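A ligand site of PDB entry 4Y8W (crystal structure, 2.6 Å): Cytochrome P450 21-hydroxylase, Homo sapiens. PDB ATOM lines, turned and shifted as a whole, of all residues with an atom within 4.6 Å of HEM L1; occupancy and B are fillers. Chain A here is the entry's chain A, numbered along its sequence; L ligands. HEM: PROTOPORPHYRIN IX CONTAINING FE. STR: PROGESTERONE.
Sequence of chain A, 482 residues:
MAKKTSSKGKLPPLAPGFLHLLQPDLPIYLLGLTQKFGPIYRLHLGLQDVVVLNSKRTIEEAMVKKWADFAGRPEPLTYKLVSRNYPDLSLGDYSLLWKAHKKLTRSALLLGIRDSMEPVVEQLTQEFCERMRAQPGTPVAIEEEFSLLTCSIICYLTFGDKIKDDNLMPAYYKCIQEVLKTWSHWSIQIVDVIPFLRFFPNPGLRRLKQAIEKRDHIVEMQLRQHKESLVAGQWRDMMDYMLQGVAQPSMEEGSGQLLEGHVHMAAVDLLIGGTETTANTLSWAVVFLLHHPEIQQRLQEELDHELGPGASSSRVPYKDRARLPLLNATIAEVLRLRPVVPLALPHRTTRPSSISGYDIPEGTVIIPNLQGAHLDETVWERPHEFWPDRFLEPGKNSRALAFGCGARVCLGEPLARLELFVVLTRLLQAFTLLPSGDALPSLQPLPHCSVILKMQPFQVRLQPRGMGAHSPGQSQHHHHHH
O of Ser 90 sits close to O1D of HEM L1 (3.3 Å).
The backbone carbonyl oxygen of Gly 273 lies close to a nitrogen (NC) of HEM L1 (3.1 Å).
CZ2 of Trp 98 touches O2D of HEM L1 (3.7 Å).
CD1 of Ile 154 touches CBC of HEM L1 (3.5 Å).
CB of Asp 269 touches CMD of HEM L1, at 3.9 Å.
O of Leu 270 touches CAC of HEM L1 (3.7 Å).
Gly 274 touches HEM L1.
Thr 277 touches HEM L1 (OG1 to CHC, 3.2 Å).
Thr 278 touches HEM L1.
Thr 281 touches HEM L1.
Leu 335 touches HEM L1.
Val 340 touches HEM L1.
Val 341 touches HEM L1 (CG2 to CHB, 3.7 Å).
Ala 344 touches HEM L1.
Leu 345 touches HEM L1 (N to O1A, 3.7 Å).
Leu 370 touches HEM L1.
Ala 402 touches HEM L1 (O to CMB, 3.3 Å).
Phe 403 touches HEM L1.
CB of Leu 411 touches CMD of HEM L1, 3.6 Å away.
Gly 412 touches HEM L1 (CA to C3C, 3.5 Å).
Leu 415 touches HEM L1.
CB of Ala 416 touches CHC of HEM L1 (3.9 Å).
Hydrophobic or aromatic side chains that line HEM L1: Trp 98, Ile 154, Leu 335, Val 340, Val 341, Ala 344, Leu 345, His 347, Leu 370, Phe 403, Leu 411, Leu 415 and Ala 416.
Of the 33 residues printed, 27 come within 4 Å of HEM L1.
The backbone carbonyl oxygen (O) of Gly 273 lies within hydrogen-bond range of the side-chain hydroxyl (OG1) of Thr 277 (2.6 Å).
N of Ser 90 sits at hydrogen-bond distance from OD2 of Asp 269, at 2.9 Å.
NE1 of Trp 98 sits at hydrogen-bond distance from O of Leu 89, 2.7 Å away.
NE of Arg 73 lies within hydrogen-bond range of O of Ser 90.
The backbone carbonyl oxygen (O) of Ala 407 is in hydrogen-bond range of the side-chain amino group (NZ) of Lys 102 (2.9 Å).
O of Leu 89 lies within hydrogen-bond range of NH2 of Arg 408, at 3.1 Å.
OG1 of Thr 281 sits at hydrogen-bond distance from O of Thr 277 (2.8 Å).
N of Cys 410 lies within hydrogen-bond range of O of Phe 403, at 3.1 Å.
O1D of HEM L1 lies within salt-bridge range of NH2 of Arg 408 (2.9 Å).
An oxygen (O2A) of HEM L1 lies within hydrogen-bond range of a ring nitrogen (NE2) of His 347 (2.8 Å).
SG of Cys 410 is bound to FE of HEM L1 (2.2 Å).
NZ of Lys 102 lies within salt-bridge range of O2D of HEM L1, at 2.8 Å.
O1D of HEM L1 lies within salt-bridge range of NH2 of Arg 73.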
ATOM      1  N   ARG A  73      19.002 -18.009 -18.668  1.00  0.00           N
ATOM      2  CA  ARG A  73      19.686 -17.314 -17.569  1.00  0.00           C
ATOM      3  C   ARG A  73      20.280 -18.333 -16.583  1.00  0.00           C
ATOM      4  O   ARG A  73      19.756 -19.445 -16.461  1.00  0.00           O
ATOM      5  CB  ARG A  73      18.723 -16.377 -16.832  1.00  0.00           C
ATOM      6  CG  ARG A  73      18.282 -15.145 -17.613  1.00  0.00           C
ATOM      7  CD  ARG A  73      19.230 -13.968 -17.458  1.00  0.00           C
ATOM      8  NE  ARG A  73      18.762 -12.788 -18.184  1.00  0.00           N
ATOM      9  CZ  ARG A  73      19.371 -12.226 -19.230  1.00  0.00           C
ATOM     10  NH1 ARG A  73      20.513 -12.715 -19.698  1.00  0.00           N
ATOM     11  NH2 ARG A  73      18.836 -11.153 -19.804  1.00  0.00           N
ATOM     12  N   LEU A  89      11.196 -11.715 -14.828  1.00  0.00           N
ATOM     13  CA  LEU A  89      11.352 -11.720 -16.274  1.00  0.00           C
ATOM     14  C   LEU A  89      12.841 -11.641 -16.629  1.00  0.00           C
ATOM     15  O   LEU A  89      13.360 -12.541 -17.297  1.00  0.00           O
ATOM     16  CB  LEU A  89      10.530 -10.580 -16.892  1.00  0.00           C
ATOM     17  CG  LEU A  89      10.766  -9.830 -18.218  1.00  0.00           C
ATOM     18  CD1 LEU A  89      11.303 -10.654 -19.369  1.00  0.00           C
ATOM     19  CD2 LEU A  89       9.462  -9.164 -18.619  1.00  0.00           C
ATOM     20  N   SER A  90      13.515 -10.598 -16.155  1.00  0.00           N
ATOM     21  CA  SER A  90      14.892 -10.286 -16.532  1.00  0.00           C
ATOM     22  C   SER A  90      15.908 -11.353 -16.118  1.00  0.00           C
ATOM     23  O   SER A  90      16.925 -11.539 -16.797  1.00  0.00           O
ATOM     24  CB  SER A  90      15.301  -8.927 -15.969  1.00  0.00           C
ATOM     25  OG  SER A  90      15.396  -8.955 -14.564  1.00  0.00           O
ATOM     26  N   TRP A  98       8.031 -18.048 -19.861  1.00  0.00           N
ATOM     27  CA  TRP A  98       8.836 -16.814 -19.861  1.00  0.00           C
ATOM     28  C   TRP A  98       8.585 -15.968 -21.121  1.00  0.00           C
ATOM     29  O   TRP A  98       8.543 -14.731 -21.036  1.00  0.00           O
ATOM     30  CB  TRP A  98      10.333 -17.115 -19.710  1.00  0.00           C
ATOM     31  CG  TRP A  98      11.186 -15.890 -19.846  1.00  0.00           C
ATOM     32  CD1 TRP A  98      11.581 -15.045 -18.849  1.00  0.00           C
ATOM     33  CD2 TRP A  98      11.726 -15.358 -21.065  1.00  0.00           C
ATOM     34  NE1 TRP A  98      12.323 -14.016 -19.363  1.00  0.00           N
ATOM     35  CE2 TRP A  98      12.432 -14.179 -20.724  1.00  0.00           C
ATOM     36  CE3 TRP A  98      11.682 -15.753 -22.408  1.00  0.00           C
ATOM     37  CZ2 TRP A  98      13.094 -13.390 -21.684  1.00  0.00           C
ATOM     38  CZ3 TRP A  98      12.331 -14.969 -23.367  1.00  0.00           C
ATOM     39  CH2 TRP A  98      13.028 -13.802 -22.997  1.00  0.00           C
ATOM     40  N   LYS A 102       7.313 -12.137 -21.114  1.00  0.00           N
ATOM     41  CA  LYS A 102       7.946 -10.991 -21.790  1.00  0.00           C
ATOM     42  C   LYS A 102       7.033 -10.348 -22.848  1.00  0.00           C
ATOM     43  O   LYS A 102       6.910  -9.123 -22.887  1.00  0.00           O
ATOM     44  CB  LYS A 102       9.298 -11.362 -22.395  1.00  0.00           C
ATOM     45  CG  LYS A 102      10.053 -10.178 -22.971  1.00  0.00           C
ATOM     46  CD  LYS A 102      11.519 -10.452 -23.198  1.00  0.00           C
ATOM     47  CE  LYS A 102      12.189  -9.268 -23.885  1.00  0.00           C
ATOM     48  NZ  LYS A 102      13.664  -9.454 -23.998  1.00  0.00           N
ATOM     49  N   ILE A 154       9.144   6.332 -15.565  1.00  0.00           N
ATOM     50  CA  ILE A 154       8.785   4.906 -15.493  1.00  0.00           C
ATOM     51  C   ILE A 154       7.712   4.609 -14.445  1.00  0.00           C
ATOM     52  O   ILE A 154       6.884   3.713 -14.642  1.00  0.00           O
ATOM     53  CB  ILE A 154      10.033   3.964 -15.408  1.00  0.00           C
ATOM     54  CG1 ILE A 154       9.665   2.484 -15.587  1.00  0.00           C
ATOM     55  CG2 ILE A 154      10.803   4.162 -14.109  1.00  0.00           C
ATOM     56  CD1 ILE A 154       9.012   2.139 -16.914  1.00  0.00           C
ATOM     57  N   ASP A 269      10.863  -5.091 -12.731  1.00  0.00           N
ATOM     58  CA  ASP A 269      11.848  -5.077 -13.816  1.00  0.00           C
ATOM     59  C   ASP A 269      11.789  -3.788 -14.650  1.00  0.00           C
ATOM     60  O   ASP A 269      12.841  -3.247 -15.014  1.00  0.00           O
ATOM     61  CB  ASP A 269      11.681  -6.317 -14.703  1.00  0.00           C
ATOM     62  CG  ASP A 269      12.034  -7.604 -13.985  1.00  0.00           C
ATOM     63  OD1 ASP A 269      12.323  -7.559 -12.771  1.00  0.00           O
ATOM     64  OD2 ASP A 269      12.015  -8.685 -14.620  1.00  0.00           O
ATOM     65  N   LEU A 270      10.582  -3.324 -14.938  1.00  0.00           N
ATOM     66  CA  LEU A 270      10.346  -1.999 -15.521  1.00  0.00           C
ATOM     67  C   LEU A 270      10.940  -0.888 -14.653  1.00  0.00           C
ATOM     68  O   LEU A 270      11.742  -0.093 -15.135  1.00  0.00           O
ATOM     69  CB  LEU A 270       8.842  -1.760 -15.724  1.00  0.00           C
ATOM     70  CG  LEU A 270       8.107  -1.836 -17.077  1.00  0.00           C
ATOM     71  CD1 LEU A 270       8.888  -2.507 -18.206  1.00  0.00           C
ATOM     72  CD2 LEU A 270       6.758  -2.520 -16.869  1.00  0.00           C
ATOM     73  N   GLY A 273      14.983  -1.530 -13.879  1.00  0.00           N
ATOM     74  CA  GLY A 273      15.648  -1.541 -15.185  1.00  0.00           C
ATOM     75  C   GLY A 273      15.560  -0.227 -15.942  1.00  0.00           C
ATOM     76  O   GLY A 273      16.359   0.012 -16.848  1.00  0.00           O
ATOM     77  N   GLY A 274      14.606   0.613 -15.560  1.00  0.00           N
ATOM     78  CA  GLY A 274      14.294   1.840 -16.288  1.00  0.00           C
ATOM     79  C   GLY A 274      14.790   3.160 -15.746  1.00  0.00           C
ATOM     80  O   GLY A 274      14.729   4.170 -16.465  1.00  0.00           O
ATOM     81  N   THR A 277      19.618   3.256 -15.712  1.00  0.00           N
ATOM     82  CA  THR A 277      20.159   2.990 -17.050  1.00  0.00           C
ATOM     83  C   THR A 277      20.074   4.217 -17.978  1.00  0.00           C
ATOM     84  O   THR A 277      21.076   4.646 -18.551  1.00  0.00           O
ATOM     85  CB  THR A 277      19.483   1.780 -17.723  1.00  0.00           C
ATOM     86  OG1 THR A 277      18.061   1.871 -17.569  1.00  0.00           O
ATOM     87  CG2 THR A 277      19.983   0.473 -17.129  1.00  0.00           C
ATOM     88  N   THR A 278      18.873   4.783 -18.097  1.00  0.00           N
ATOM     89  CA  THR A 278      18.638   5.960 -18.937  1.00  0.00           C
ATOM     90  C   THR A 278      19.220   7.235 -18.323  1.00  0.00           C
ATOM     91  O   THR A 278      19.642   8.129 -19.063  1.00  0.00           O
ATOM     92  CB  THR A 278      17.137   6.172 -19.252  1.00  0.00           C
ATOM     93  OG1 THR A 278      16.354   5.902 -18.088  1.00  0.00           O
ATOM     94  CG2 THR A 278      16.690   5.252 -20.368  1.00  0.00           C
ATOM     95  N   THR A 281      23.129   7.098 -18.949  1.00  0.00           N
ATOM     96  CA  THR A 281      23.353   7.366 -20.376  1.00  0.00           C
ATOM     97  C   THR A 281      23.270   8.867 -20.645  1.00  0.00           C
ATOM     98  O   THR A 281      24.131   9.423 -21.338  1.00  0.00           O
ATOM     99  CB  THR A 281      22.365   6.582 -21.273  1.00  0.00           C
ATOM    100  OG1 THR A 281      22.396   5.196 -20.905  1.00  0.00           O
ATOM    101  CG2 THR A 281      22.741   6.706 -22.751  1.00  0.00           C
ATOM    102  N   LEU A 335      25.867   5.744 -26.597  1.00  0.00           N
ATOM    103  CA  LEU A 335      25.473   4.340 -26.455  1.00  0.00           C
ATOM    104  C   LEU A 335      26.571   3.372 -26.903  1.00  0.00           C
ATOM    105  O   LEU A 335      26.783   2.335 -26.279  1.00  0.00           O
ATOM    106  CB  LEU A 335      24.165   4.058 -27.225  1.00  0.00           C
ATOM    107  CG  LEU A 335      22.844   4.677 -26.734  1.00  0.00           C
ATOM    108  CD1 LEU A 335      21.793   4.620 -27.837  1.00  0.00           C
ATOM    109  CD2 LEU A 335      22.325   4.016 -25.470  1.00  0.00           C
ATOM    110  N   VAL A 340      25.655   1.605 -20.992  1.00  0.00           N
ATOM    111  CA  VAL A 340      25.358   1.679 -19.561  1.00  0.00           C
ATOM    112  C   VAL A 340      25.251   0.307 -18.864  1.00  0.00           C
ATOM    113  O   VAL A 340      25.430   0.216 -17.648  1.00  0.00           O
ATOM    114  CB  VAL A 340      24.130   2.598 -19.289  1.00  0.00           C
ATOM    115  CG1 VAL A 340      22.815   1.850 -19.446  1.00  0.00           C
ATOM    116  CG2 VAL A 340      24.227   3.248 -17.919  1.00  0.00           C
ATOM    117  N   VAL A 341      24.977  -0.744 -19.649  1.00  0.00           N
ATOM    118  CA  VAL A 341      25.046  -2.129 -19.183  1.00  0.00           C
ATOM    119  C   VAL A 341      26.156  -2.830 -19.994  1.00  0.00           C
ATOM    120  O   VAL A 341      25.857  -3.553 -20.954  1.00  0.00           O
ATOM    121  CB  VAL A 341      23.667  -2.846 -19.276  1.00  0.00           C
ATOM    122  CG1 VAL A 341      23.686  -4.180 -18.529  1.00  0.00           C
ATOM    123  CG2 VAL A 341      22.546  -1.970 -18.728  1.00  0.00           C
ATOM    124  N   ALA A 344      26.192  -6.698 -20.545  1.00  0.00           N
ATOM    125  CA  ALA A 344      24.791  -7.149 -20.603  1.00  0.00           C
ATOM    126  C   ALA A 344      24.373  -7.839 -19.290  1.00  0.00           C
ATOM    127  O   ALA A 344      24.765  -7.395 -18.204  1.00  0.00           O
ATOM    128  CB  ALA A 344      24.548  -8.039 -21.821  1.00  0.00           C
ATOM    129  N   LEU A 345      23.576  -8.912 -19.395  1.00  0.00           N
ATOM    130  CA  LEU A 345      23.310  -9.822 -18.290  1.00  0.00           C
ATOM    131  C   LEU A 345      23.803 -11.220 -18.689  1.00  0.00           C
ATOM    132  O   LEU A 345      23.910 -11.493 -19.885  1.00  0.00           O
ATOM    133  CB  LEU A 345      21.821  -9.847 -17.946  1.00  0.00           C
ATOM    134  CG  LEU A 345      21.221  -8.852 -16.942  1.00  0.00           C
ATOM    135  CD1 LEU A 345      21.960  -8.807 -15.608  1.00  0.00           C
ATOM    136  CD2 LEU A 345      21.117  -7.458 -17.542  1.00  0.00           C
ATOM    137  N   HIS A 347      24.070 -14.971 -19.854  1.00  0.00           N
ATOM    138  CA  HIS A 347      23.265 -15.908 -20.645  1.00  0.00           C
ATOM    139  C   HIS A 347      23.657 -17.345 -20.314  1.00  0.00           C
ATOM    140  O   HIS A 347      24.829 -17.629 -20.054  1.00  0.00           O
ATOM    141  CB  HIS A 347      23.471 -15.664 -22.148  1.00  0.00           C
ATOM    142  CG  HIS A 347      22.833 -14.413 -22.648  1.00  0.00           C
ATOM    143  ND1 HIS A 347      21.786 -14.411 -23.542  1.00  0.00           N
ATOM    144  CD2 HIS A 347      23.113 -13.111 -22.409  1.00  0.00           C
ATOM    145  CE1 HIS A 347      21.439 -13.170 -23.816  1.00  0.00           C
ATOM    146  NE2 HIS A 347      22.222 -12.360 -23.135  1.00  0.00           N
ATOM    147  N   LEU A 370      29.586  -6.118 -24.250  1.00  0.00           N
ATOM    148  CA  LEU A 370      29.082  -5.098 -25.161  1.00  0.00           C
ATOM    149  C   LEU A 370      30.037  -3.919 -25.347  1.00  0.00           C
ATOM    150  O   LEU A 370      30.222  -3.463 -26.483  1.00  0.00           O
ATOM    151  CB  LEU A 370      27.678  -4.620 -24.755  1.00  0.00           C
ATOM    152  CG  LEU A 370      26.543  -5.656 -24.689  1.00  0.00           C
ATOM    153  CD1 LEU A 370      25.296  -4.999 -24.111  1.00  0.00           C
ATOM    154  CD2 LEU A 370      26.215  -6.319 -26.029  1.00  0.00           C
ATOM    155  N   ALA A 402      24.074  -1.520 -27.597  1.00  0.00           N
ATOM    156  CA  ALA A 402      23.987  -1.114 -26.187  1.00  0.00           C
ATOM    157  C   ALA A 402      22.798  -1.781 -25.467  1.00  0.00           C
ATOM    158  O   ALA A 402      22.791  -1.888 -24.237  1.00  0.00           O
ATOM    159  CB  ALA A 402      23.902   0.402 -26.066  1.00  0.00           C
ATOM    160  N   PHE A 403      21.816  -2.225 -26.256  1.00  0.00           N
ATOM    161  CA  PHE A 403      20.594  -2.856 -25.766  1.00  0.00           C
ATOM    162  C   PHE A 403      20.590  -4.371 -25.947  1.00  0.00           C
ATOM    163  O   PHE A 403      19.599  -5.042 -25.624  1.00  0.00           O
ATOM    164  CB  PHE A 403      19.389  -2.256 -26.505  1.00  0.00           C
ATOM    165  CG  PHE A 403      19.184  -0.796 -26.248  1.00  0.00           C
ATOM    166  CD1 PHE A 403      18.447  -0.370 -25.143  1.00  0.00           C
ATOM    167  CD2 PHE A 403      19.710   0.159 -27.111  1.00  0.00           C
ATOM    168  CE1 PHE A 403      18.242   0.980 -24.906  1.00  0.00           C
ATOM    169  CE2 PHE A 403      19.518   1.514 -26.874  1.00  0.00           C
ATOM    170  CZ  PHE A 403      18.778   1.928 -25.775  1.00  0.00           C
ATOM    171  N   GLY A 404      21.699  -4.900 -26.467  1.00  0.00           N
ATOM    172  CA  GLY A 404      21.811  -6.319 -26.802  1.00  0.00           C
ATOM    173  C   GLY A 404      21.037  -6.659 -28.054  1.00  0.00           C
ATOM    174  O   GLY A 404      20.614  -5.779 -28.807  1.00  0.00           O
ATOM    175  N   ALA A 407      16.500 -12.827 -28.213  1.00  0.00           N
ATOM    176  CA  ALA A 407      15.390 -13.038 -27.263  1.00  0.00           C
ATOM    177  C   ALA A 407      15.476 -12.201 -25.979  1.00  0.00           C
ATOM    178  O   ALA A 407      14.449 -11.914 -25.357  1.00  0.00           O
ATOM    179  CB  ALA A 407      15.243 -14.516 -26.925  1.00  0.00           C
ATOM    180  N   ARG A 408      16.693 -11.811 -25.598  1.00  0.00           N
ATOM    181  CA  ARG A 408      16.929 -11.075 -24.353  1.00  0.00           C
ATOM    182  C   ARG A 408      17.131  -9.573 -24.532  1.00  0.00           C
ATOM    183  O   ARG A 408      17.550  -8.896 -23.579  1.00  0.00           O
ATOM    184  CB  ARG A 408      18.088 -11.702 -23.553  1.00  0.00           C
ATOM    185  CG  ARG A 408      17.979 -13.198 -23.228  1.00  0.00           C
ATOM    186  CD  ARG A 408      16.619 -13.613 -22.694  1.00  0.00           C
ATOM    187  NE  ARG A 408      16.319 -13.055 -21.373  1.00  0.00           N
ATOM    188  CZ  ARG A 408      16.065 -13.764 -20.277  1.00  0.00           C
ATOM    189  NH1 ARG A 408      16.055 -15.086 -20.311  1.00  0.00           N
ATOM    190  NH2 ARG A 408      15.795 -13.129 -19.149  1.00  0.00           N
ATOM    191  N   VAL A 409      16.819  -9.034 -25.722  1.00  0.00           N
ATOM    192  CA  VAL A 409      16.850  -7.579 -25.977  1.00  0.00           C
ATOM    193  C   VAL A 409      16.215  -6.799 -24.841  1.00  0.00           C
ATOM    194  O   VAL A 409      15.191  -7.217 -24.296  1.00  0.00           O
ATOM    195  CB  VAL A 409      16.135  -7.129 -27.289  1.00  0.00           C
ATOM    196  CG1 VAL A 409      17.065  -7.179 -28.480  1.00  0.00           C
ATOM    197  CG2 VAL A 409      14.819  -7.872 -27.538  1.00  0.00           C
ATOM    198  N   CYS A 410      16.827  -5.672 -24.513  1.00  0.00           N
ATOM    199  CA  CYS A 410      16.293  -4.758 -23.519  1.00  0.00           C
ATOM    200  C   CYS A 410      14.798  -4.528 -23.757  1.00  0.00           C
ATOM    201  O   CYS A 410      14.388  -4.159 -24.867  1.00  0.00           O
ATOM    202  CB  CYS A 410      17.038  -3.434 -23.582  1.00  0.00           C
ATOM    203  SG  CYS A 410      16.481  -2.282 -22.322  1.00  0.00           S
ATOM    204  N   LEU A 411      14.003  -4.790 -22.722  1.00  0.00           N
ATOM    205  CA  LEU A 411      12.552  -4.649 -22.777  1.00  0.00           C
ATOM    206  C   LEU A 411      12.149  -3.189 -23.017  1.00  0.00           C
ATOM    207  O   LEU A 411      11.177  -2.921 -23.716  1.00  0.00           O
ATOM    208  CB  LEU A 411      11.927  -5.168 -21.464  1.00  0.00           C
ATOM    209  CG  LEU A 411      10.446  -5.571 -21.267  1.00  0.00           C
ATOM    210  CD1 LEU A 411       9.463  -4.406 -21.251  1.00  0.00           C
ATOM    211  CD2 LEU A 411       9.982  -6.611 -22.274  1.00  0.00           C
ATOM    212  N   GLY A 412      12.919  -2.261 -22.445  1.00  0.00           N
ATOM    213  CA  GLY A 412      12.562  -0.851 -22.448  1.00  0.00           C
ATOM    214  C   GLY A 412      13.241   0.028 -23.487  1.00  0.00           C
ATOM    215  O   GLY A 412      13.124   1.242 -23.405  1.00  0.00           O
ATOM    216  N   LEU A 415      11.101   2.946 -25.144  1.00  0.00           N
ATOM    217  CA  LEU A 415      10.919   3.995 -24.137  1.00  0.00           C
ATOM    218  C   LEU A 415      12.237   4.682 -23.769  1.00  0.00           C
ATOM    219  O   LEU A 415      12.253   5.870 -23.491  1.00  0.00           O
ATOM    220  CB  LEU A 415      10.216   3.415 -22.894  1.00  0.00           C
ATOM    221  CG  LEU A 415       9.747   4.252 -21.683  1.00  0.00           C
ATOM    222  CD1 LEU A 415      10.750   4.192 -20.548  1.00  0.00           C
ATOM    223  CD2 LEU A 415       9.345   5.695 -22.022  1.00  0.00           C
ATOM    224  N   ALA A 416      13.337   3.919 -23.794  1.00  0.00           N
ATOM    225  CA  ALA A 416      14.681   4.448 -23.492  1.00  0.00           C
ATOM    226  C   ALA A 416      15.175   5.464 -24.536  1.00  0.00           C
ATOM    227  O   ALA A 416      15.659   6.536 -24.172  1.00  0.00           O
ATOM    228  CB  ALA A 416      15.678   3.312 -23.341  1.00  0.00           C
ATOM    229  N   GLU A 419      13.256   8.792 -24.324  1.00  0.00           N
ATOM    230  CA  GLU A 419      13.729   9.602 -23.207  1.00  0.00           C
ATOM    231  C   GLU A 419      15.010  10.343 -23.587  1.00  0.00           C
ATOM    232  O   GLU A 419      15.110  11.543 -23.355  1.00  0.00           O
ATOM    233  CB  GLU A 419      13.947   8.741 -21.951  1.00  0.00           C
ATOM    234  CG  GLU A 419      12.678   8.266 -21.280  1.00  0.00           C
ATOM    235  CD  GLU A 419      12.953   7.509 -20.000  1.00  0.00           C
ATOM    236  OE1 GLU A 419      13.084   6.270 -20.052  1.00  0.00           O
ATOM    237  OE2 GLU A 419      13.081   8.163 -18.936  1.00  0.00           O
ATOM    238  N   LEU A 420      15.956   9.626 -24.193  1.00  0.00           N
ATOM    239  CA  LEU A 420      17.236  10.221 -24.619  1.00  0.00           C
ATOM    240  C   LEU A 420      17.038  11.336 -25.647  1.00  0.00           C
ATOM    241  O   LEU A 420      17.724  12.357 -25.583  1.00  0.00           O
ATOM    242  CB  LEU A 420      18.185   9.139 -25.144  1.00  0.00           C
ATOM    243  CG  LEU A 420      18.603   8.007 -24.179  1.00  0.00           C
ATOM    244  CD1 LEU A 420      19.370   6.917 -24.925  1.00  0.00           C
ATOM    245  CD2 LEU A 420      19.399   8.516 -22.991  1.00  0.00           C
HETATM  246  CHA HEM L   1      17.809  -5.779 -20.314  1.00  0.00           C
HETATM  247  CHB HEM L   1      20.520  -2.053 -21.783  1.00  0.00           C
HETATM  248  CHC HEM L   1      16.956   1.032 -20.501  1.00  0.00           C
HETATM  249  CHD HEM L   1      14.375  -2.711 -18.837  1.00  0.00           C
HETATM  250  C1A HEM L   1      18.830  -5.031 -20.829  1.00  0.00           C
HETATM  251  C2A HEM L   1      20.031  -5.574 -21.344  1.00  0.00           C
HETATM  252  C3A HEM L   1      20.792  -4.518 -21.754  1.00  0.00           C
HETATM  253  C4A HEM L   1      20.065  -3.333 -21.506  1.00  0.00           C
HETATM  254  CMA HEM L   1      22.171  -4.582 -22.363  1.00  0.00           C
HETATM  255  CAA HEM L   1      20.371  -7.058 -21.376  1.00  0.00           C
HETATM  256  CBA HEM L   1      20.524  -7.696 -22.763  1.00  0.00           C
HETATM  257  CGA HEM L   1      20.961  -9.150 -22.652  1.00  0.00           C
HETATM  258  O1A HEM L   1      20.779  -9.819 -21.604  1.00  0.00           O
HETATM  259  O2A HEM L   1      21.498  -9.701 -23.640  1.00  0.00           O
HETATM  260  C1B HEM L   1      19.766  -0.883 -21.562  1.00  0.00           C
HETATM  261  C2B HEM L   1      20.254   0.419 -21.897  1.00  0.00           C
HETATM  262  C3B HEM L   1      19.275   1.312 -21.547  1.00  0.00           C
HETATM  263  C4B HEM L   1      18.158   0.492 -20.973  1.00  0.00           C
HETATM  264  CMB HEM L   1      21.601   0.722 -22.543  1.00  0.00           C
HETATM  265  CAB HEM L   1      19.256   2.797 -21.674  1.00  0.00           C
HETATM  266  CBB HEM L   1      19.628   3.448 -22.770  1.00  0.00           C
HETATM  267  C1C HEM L   1      15.888   0.284 -19.999  1.00  0.00           C
HETATM  268  C2C HEM L   1      14.582   0.764 -19.724  1.00  0.00           C
HETATM  269  C3C HEM L   1      13.846  -0.320 -19.234  1.00  0.00           C
HETATM  270  C4C HEM L   1      14.719  -1.446 -19.250  1.00  0.00           C
HETATM  271  CMC HEM L   1      14.128   2.205 -19.919  1.00  0.00           C
HETATM  272  CAC HEM L   1      12.424  -0.395 -18.782  1.00  0.00           C
HETATM  273  CBC HEM L   1      11.541   0.600 -18.855  1.00  0.00           C
HETATM  274  C1D HEM L   1      15.136  -3.840 -19.133  1.00  0.00           C
HETATM  275  C2D HEM L   1      14.648  -5.196 -18.799  1.00  0.00           C
HETATM  276  C3D HEM L   1      15.612  -6.046 -19.217  1.00  0.00           C
HETATM  277  C4D HEM L   1      16.670  -5.198 -19.791  1.00  0.00           C
HETATM  278  CMD HEM L   1      13.344  -5.555 -18.123  1.00  0.00           C
HETATM  279  CAD HEM L   1      15.635  -7.564 -19.122  1.00  0.00           C
HETATM  280  CBD HEM L   1      14.997  -8.193 -20.363  1.00  0.00           C
HETATM  281  CGD HEM L   1      15.339  -9.654 -20.560  1.00  0.00           C
HETATM  282  O1D HEM L   1      16.003 -10.312 -19.727  1.00  0.00           O
HETATM  283  O2D HEM L   1      14.966 -10.240 -21.607  1.00  0.00           O
HETATM  284  NA  HEM L   1      18.878  -3.656 -20.907  1.00  0.00           N
HETATM  285  NB  HEM L   1      18.543  -0.797 -21.016  1.00  0.00           N
HETATM  286  NC  HEM L   1      15.938  -1.056 -19.721  1.00  0.00           N
HETATM  287  ND  HEM L   1      16.341  -3.892 -19.723  1.00  0.00           N
HETATM  288 FE   HEM L   1      17.391  -2.437 -20.346  1.00  0.00          FE
HETATM  289  C1  STR L   2      17.890  -5.731  -8.772  1.00  0.00           C
HETATM  290  C2  STR L   2      17.414  -6.302  -7.431  1.00  0.00           C
HETATM  291  C3  STR L   2      15.939  -6.600  -7.491  1.00  0.00           C
HETATM  292  O3  STR L   2      15.253  -6.552  -6.485  1.00  0.00           O
HETATM  293  C4  STR L   2      15.323  -6.970  -8.782  1.00  0.00           C
HETATM  294  C5  STR L   2      15.998  -6.966  -9.941  1.00  0.00           C
HETATM  295  C6  STR L   2      15.241  -7.429 -11.177  1.00  0.00           C
HETATM  296  C7  STR L   2      15.438  -6.419 -12.309  1.00  0.00           C
HETATM  297  C8  STR L   2      16.927  -6.147 -12.552  1.00  0.00           C
HETATM  298  C9  STR L   2      17.587  -5.560 -11.267  1.00  0.00           C
HETATM  299  C10 STR L   2      17.465  -6.497 -10.036  1.00  0.00           C
HETATM  300  C11 STR L   2      19.013  -4.987 -11.511  1.00  0.00           C
HETATM  301  C12 STR L   2      19.230  -4.210 -12.817  1.00  0.00           C
HETATM  302  C13 STR L   2      18.663  -4.927 -14.038  1.00  0.00           C
HETATM  303  C14 STR L   2      17.185  -5.236 -13.757  1.00  0.00           C
HETATM  304  C15 STR L   2      16.532  -5.549 -15.101  1.00  0.00           C
HETATM  305  C16 STR L   2      17.303  -4.658 -16.073  1.00  0.00           C
HETATM  306  C17 STR L   2      18.484  -4.048 -15.282  1.00  0.00           C
HETATM  307  C18 STR L   2      19.538  -6.161 -14.365  1.00  0.00           C
HETATM  308  C19 STR L   2      18.343  -7.761 -10.183  1.00  0.00           C
HETATM  309  C20 STR L   2      19.717  -3.765 -16.121  1.00  0.00           C
HETATM  310  O20 STR L   2      20.680  -3.214 -15.595  1.00  0.00           O
HETATM  311  C21 STR L   2      19.777  -4.131 -17.570  1.00  0.00           C
